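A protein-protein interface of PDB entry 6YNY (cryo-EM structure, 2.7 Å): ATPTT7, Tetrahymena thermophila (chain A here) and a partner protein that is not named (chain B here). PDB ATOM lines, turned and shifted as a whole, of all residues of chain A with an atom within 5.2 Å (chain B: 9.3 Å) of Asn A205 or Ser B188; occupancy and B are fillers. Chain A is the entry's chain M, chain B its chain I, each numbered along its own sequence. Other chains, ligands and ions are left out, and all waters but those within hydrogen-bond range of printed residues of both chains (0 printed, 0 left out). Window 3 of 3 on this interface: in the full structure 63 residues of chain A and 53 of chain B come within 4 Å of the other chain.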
ATOM      1  N   ARG A 201      24.975  -1.876 -12.895  1.00  0.00           N
ATOM      2  CA  ARG A 201      23.717  -2.539 -13.202  1.00  0.00           C
ATOM      3  C   ARG A 201      23.838  -3.494 -14.379  1.00  0.00           C
ATOM      4  O   ARG A 201      22.946  -4.324 -14.579  1.00  0.00           O
ATOM      5  CB  ARG A 201      22.640  -1.492 -13.487  1.00  0.00           C
ATOM      6  CG  ARG A 201      21.237  -2.040 -13.495  1.00  0.00           C
ATOM      7  CD  ARG A 201      20.206  -0.968 -13.794  1.00  0.00           C
ATOM      8  NE  ARG A 201      20.282   0.158 -12.869  1.00  0.00           N
ATOM      9  CZ  ARG A 201      20.906   1.304 -13.121  1.00  0.00           C
ATOM     10  NH1 ARG A 201      21.521   1.501 -14.279  1.00  0.00           N
ATOM     11  NH2 ARG A 201      20.911   2.262 -12.209  1.00  0.00           N
ATOM     12  N   TYR A 203      26.429  -5.680 -14.802  1.00  0.00           N
ATOM     13  CA  TYR A 203      27.071  -6.914 -14.370  1.00  0.00           C
ATOM     14  C   TYR A 203      26.550  -7.407 -13.027  1.00  0.00           C
ATOM     15  O   TYR A 203      27.078  -8.388 -12.492  1.00  0.00           O
ATOM     16  CB  TYR A 203      28.587  -6.724 -14.312  1.00  0.00           C
ATOM     17  CG  TYR A 203      29.197  -6.425 -15.656  1.00  0.00           C
ATOM     18  CD1 TYR A 203      29.463  -7.442 -16.555  1.00  0.00           C
ATOM     19  CD2 TYR A 203      29.499  -5.128 -16.032  1.00  0.00           C
ATOM     20  CE1 TYR A 203      30.013  -7.177 -17.785  1.00  0.00           C
ATOM     21  CE2 TYR A 203      30.049  -4.855 -17.262  1.00  0.00           C
ATOM     22  CZ  TYR A 203      30.304  -5.883 -18.134  1.00  0.00           C
ATOM     23  OH  TYR A 203      30.854  -5.614 -19.361  1.00  0.00           O
ATOM     24  N   THR A 204      25.531  -6.758 -12.469  1.00  0.00           N
ATOM     25  CA  THR A 204      24.920  -7.188 -11.223  1.00  0.00           C
ATOM     26  C   THR A 204      23.414  -7.012 -11.321  1.00  0.00           C
ATOM     27  O   THR A 204      22.888  -6.483 -12.303  1.00  0.00           O
ATOM     28  CB  THR A 204      25.454  -6.402 -10.021  1.00  0.00           C
ATOM     29  OG1 THR A 204      25.178  -5.008 -10.194  1.00  0.00           O
ATOM     30  CG2 THR A 204      26.942  -6.607  -9.867  1.00  0.00           C
ATOM     31  N   ASN A 205      22.721  -7.469 -10.284  1.00  0.00           N
ATOM     32  CA  ASN A 205      21.277  -7.286 -10.149  1.00  0.00           C
ATOM     33  C   ASN A 205      21.012  -6.526  -8.860  1.00  0.00           C
ATOM     34  O   ASN A 205      21.039  -7.122  -7.769  1.00  0.00           O
ATOM     35  CB  ASN A 205      20.550  -8.626 -10.143  1.00  0.00           C
ATOM     36  CG  ASN A 205      19.049  -8.469 -10.160  1.00  0.00           C
ATOM     37  OD1 ASN A 205      18.528  -7.414 -10.517  1.00  0.00           O
ATOM     38  ND2 ASN A 205      18.342  -9.521  -9.774  1.00  0.00           N
ATOM     39  N   PRO A 206      20.762  -5.217  -8.920  1.00  0.00           N
ATOM     40  CA  PRO A 206      20.584  -4.454  -7.675  1.00  0.00           C
ATOM     41  C   PRO A 206      19.434  -4.948  -6.823  1.00  0.00           C
ATOM     42  O   PRO A 206      19.477  -4.801  -5.596  1.00  0.00           O
ATOM     43  CB  PRO A 206      20.340  -3.024  -8.172  1.00  0.00           C
ATOM     44  CG  PRO A 206      20.889  -2.991  -9.549  1.00  0.00           C
ATOM     45  CD  PRO A 206      20.689  -4.354 -10.109  1.00  0.00           C
ATOM     46  N   LYS A 207      18.409  -5.533  -7.432  1.00  0.00           N
ATOM     47  CA  LYS A 207      17.229  -5.981  -6.695  1.00  0.00           C
ATOM     48  C   LYS A 207      17.397  -7.412  -6.198  1.00  0.00           C
ATOM     49  O   LYS A 207      16.556  -8.281  -6.416  1.00  0.00           O
ATOM     50  CB  LYS A 207      15.988  -5.845  -7.568  1.00  0.00           C
ATOM     51  CG  LYS A 207      16.080  -6.558  -8.905  1.00  0.00           C
ATOM     52  CD  LYS A 207      14.809  -6.389  -9.718  1.00  0.00           C
ATOM     53  CE  LYS A 207      14.617  -4.948 -10.158  1.00  0.00           C
ATOM     54  NZ  LYS A 207      13.491  -4.804 -11.122  1.00  0.00           N
ATOM     55  N   ASP A 208      18.507  -7.650  -5.509  1.00  0.00           N
ATOM     56  CA  ASP A 208      18.794  -8.922  -4.869  1.00  0.00           C
ATOM     57  C   ASP A 208      19.231  -8.658  -3.436  1.00  0.00           C
ATOM     58  O   ASP A 208      19.553  -7.529  -3.057  1.00  0.00           O
ATOM     59  CB  ASP A 208      19.882  -9.704  -5.614  1.00  0.00           C
ATOM     60  CG  ASP A 208      19.417 -10.219  -6.955  1.00  0.00           C
ATOM     61  OD1 ASP A 208      18.239 -10.002  -7.305  1.00  0.00           O
ATOM     62  OD2 ASP A 208      20.232 -10.848  -7.661  1.00  0.00           O
ATOM     63  N   PRO A 211      23.707  -8.306  -4.159  1.00  0.00           N
ATOM     64  CA  PRO A 211      24.109  -8.099  -5.557  1.00  0.00           C
ATOM     65  C   PRO A 211      25.527  -8.556  -5.838  1.00  0.00           C
ATOM     66  O   PRO A 211      25.800  -9.096  -6.918  1.00  0.00           O
ATOM     67  CB  PRO A 211      23.946  -6.586  -5.737  1.00  0.00           C
ATOM     68  CG  PRO A 211      22.963  -6.193  -4.724  1.00  0.00           C
ATOM     69  CD  PRO A 211      23.207  -7.068  -3.549  1.00  0.00           C
ATOM     70  N   THR B 182      25.806  -5.720 -24.075  1.00  0.00           N
ATOM     71  CA  THR B 182      24.861  -6.774 -23.729  1.00  0.00           C
ATOM     72  C   THR B 182      25.483  -8.157 -23.732  1.00  0.00           C
ATOM     73  O   THR B 182      25.115  -8.995 -22.907  1.00  0.00           O
ATOM     74  CB  THR B 182      23.675  -6.758 -24.695  1.00  0.00           C
ATOM     75  OG1 THR B 182      24.149  -6.876 -26.042  1.00  0.00           O
ATOM     76  CG2 THR B 182      22.894  -5.470 -24.537  1.00  0.00           C
ATOM     77  N   ALA B 185      26.813  -9.673 -20.501  1.00  0.00           N
ATOM     78  CA  ALA B 185      26.161  -8.858 -19.493  1.00  0.00           C
ATOM     79  C   ALA B 185      25.175  -9.690 -18.679  1.00  0.00           C
ATOM     80  O   ALA B 185      24.837 -10.823 -19.022  1.00  0.00           O
ATOM     81  CB  ALA B 185      25.443  -7.680 -20.140  1.00  0.00           C
ATOM     82  N   HIS B 186      24.711  -9.101 -17.586  1.00  0.00           N
ATOM     83  CA  HIS B 186      23.793  -9.797 -16.705  1.00  0.00           C
ATOM     84  C   HIS B 186      22.409  -9.871 -17.349  1.00  0.00           C
ATOM     85  O   HIS B 186      21.990  -8.929 -18.029  1.00  0.00           O
ATOM     86  CB  HIS B 186      23.715  -9.081 -15.361  1.00  0.00           C
ATOM     87  CG  HIS B 186      23.289  -9.959 -14.229  1.00  0.00           C
ATOM     88  ND1 HIS B 186      21.989 -10.017 -13.778  1.00  0.00           N
ATOM     89  CD2 HIS B 186      23.996 -10.807 -13.447  1.00  0.00           C
ATOM     90  CE1 HIS B 186      21.912 -10.866 -12.771  1.00  0.00           C
ATOM     91  NE2 HIS B 186      23.116 -11.360 -12.550  1.00  0.00           N
ATOM     92  N   PRO B 187      21.678 -10.972 -17.161  1.00  0.00           N
ATOM     93  CA  PRO B 187      20.370 -11.092 -17.825  1.00  0.00           C
ATOM     94  C   PRO B 187      19.396  -9.988 -17.460  1.00  0.00           C
ATOM     95  O   PRO B 187      18.612  -9.552 -18.312  1.00  0.00           O
ATOM     96  CB  PRO B 187      19.869 -12.464 -17.357  1.00  0.00           C
ATOM     97  CG  PRO B 187      21.081 -13.199 -16.943  1.00  0.00           C
ATOM     98  CD  PRO B 187      22.010 -12.181 -16.390  1.00  0.00           C
ATOM     99  N   SER B 188      19.422  -9.519 -16.217  1.00  0.00           N
ATOM    100  CA  SER B 188      18.469  -8.521 -15.753  1.00  0.00           C
ATOM    101  C   SER B 188      18.794  -7.112 -16.227  1.00  0.00           C
ATOM    102  O   SER B 188      18.103  -6.171 -15.825  1.00  0.00           O
ATOM    103  CB  SER B 188      18.402  -8.541 -14.227  1.00  0.00           C
ATOM    104  OG  SER B 188      19.628  -8.122 -13.665  1.00  0.00           O
ATOM    105  N   TYR B 189      19.815  -6.938 -17.058  1.00  0.00           N
ATOM    106  CA  TYR B 189      20.202  -5.617 -17.533  1.00  0.00           C
ATOM    107  C   TYR B 189      19.430  -5.269 -18.797  1.00  0.00           C
ATOM    108  O   TYR B 189      19.404  -6.050 -19.754  1.00  0.00           O
ATOM    109  CB  TYR B 189      21.705  -5.562 -17.803  1.00  0.00           C
ATOM    110  CG  TYR B 189      22.154  -4.295 -18.489  1.00  0.00           C
ATOM    111  CD1 TYR B 189      22.162  -3.087 -17.816  1.00  0.00           C
ATOM    112  CD2 TYR B 189      22.583  -4.311 -19.806  1.00  0.00           C
ATOM    113  CE1 TYR B 189      22.575  -1.931 -18.435  1.00  0.00           C
ATOM    114  CE2 TYR B 189      22.996  -3.159 -20.432  1.00  0.00           C
ATOM    115  CZ  TYR B 189      22.991  -1.971 -19.740  1.00  0.00           C
ATOM    116  OH  TYR B 189      23.401  -0.811 -20.352  1.00  0.00           O
ATOM    117  N   GLN B 190      18.809  -4.094 -18.796  1.00  0.00           N
ATOM    118  CA  GLN B 190      18.126  -3.559 -19.964  1.00  0.00           C
ATOM    119  C   GLN B 190      19.009  -2.496 -20.602  1.00  0.00           C
ATOM    120  O   GLN B 190      19.364  -1.507 -19.953  1.00  0.00           O
ATOM    121  CB  GLN B 190      16.768  -2.968 -19.585  1.00  0.00           C
ATOM    122  CG  GLN B 190      15.717  -3.996 -19.213  1.00  0.00           C
ATOM    123  CD  GLN B 190      16.021  -4.695 -17.907  1.00  0.00           C
ATOM    124  OE1 GLN B 190      16.929  -4.301 -17.177  1.00  0.00           O
ATOM    125  NE2 GLN B 190      15.259  -5.738 -17.604  1.00  0.00           N
ATOM    126  N   TYR B 191      19.361  -2.704 -21.866  1.00  0.00           N
ATOM    127  CA  TYR B 191      20.262  -1.789 -22.549  1.00  0.00           C
ATOM    128  C   TYR B 191      19.560  -0.472 -22.848  1.00  0.00           C
ATOM    129  O   TYR B 191      18.437  -0.452 -23.359  1.00  0.00           O
ATOM    130  CB  TYR B 191      20.779  -2.421 -23.837  1.00  0.00           C
ATOM    131  CG  TYR B 191      21.577  -1.475 -24.703  1.00  0.00           C
ATOM    132  CD1 TYR B 191      22.828  -1.031 -24.308  1.00  0.00           C
ATOM    133  CD2 TYR B 191      21.084  -1.041 -25.923  1.00  0.00           C
ATOM    134  CE1 TYR B 191      23.560  -0.173 -25.099  1.00  0.00           C
ATOM    135  CE2 TYR B 191      21.811  -0.185 -26.720  1.00  0.00           C
ATOM    136  CZ  TYR B 191      23.048   0.246 -26.304  1.00  0.00           C
ATOM    137  OH  TYR B 191      23.776   1.100 -27.096  1.00  0.00           O
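The side-chain amide oxygen (OD1) of Asn A205 sits at hydrogen-bond distance from the side-chain hydroxyl (OG) of Ser B188 (3.4 Å).
ND2 of Asn A205 sits at hydrogen-bond distance from OD1 of Asp A208. The side-chain hydroxyl (OG) of Ser B188 sits at hydrogen-bond distance from a ring nitrogen (ND1) of His B186. The side-chain amide oxygen (OE1) of Gln B190 lies close to the backbone carbonyl oxygen (O) of Ser B188 (2.6 Å).
Among the printed residues, pairs that only touch across the chains: Arg A201 with Tyr B189 (3.6 Å), Asn A205 with His B186 (3.7 Å), Thr A204 with Ser B188 (3.9 Å) and Thr A204 with His B186 (3.9 Å).
Of the printed residues of chain B, Arg A201 touches Tyr B189. Thr A204 touches just these residues of chain B: His B186 (3.9 Å) and Ser B188 (3.9 Å). Of chain B, only His B186 and Ser B188 come within 4 Å of Asn A205. No residue of chain B comes within 4 Å of Asp A208. Of the printed residues of chain A, His B186 touches Thr A204 and Asn A205. Of chain A, only Thr A204 and Asn A205 come within 4 Å of Ser B188. Of the printed residues of chain A, Tyr B189 touches Arg A201. The nearest residue of chain B that does not touch Asn A205 is Tyr B189 (6.7 Å). The nearest residue of chain A that does not touch Ser B188 is Arg A201 (5.1 Å). The nearest printed residue of chain A that does not touch Tyr B189 is Tyr A203 (5.6 Å).
Printed residues of chain B that touch a printed residue of chain A: His B186, Ser B188 and Tyr B189. Hydrophobic or aromatic side chains of chain B within 4 Å of the printed part of chain A: His B186 and Tyr B189. Among the printed residues, no Asp or Glu carboxylate lies within 4 Å of a Lys or Arg side-chain nitrogen of the other chain.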
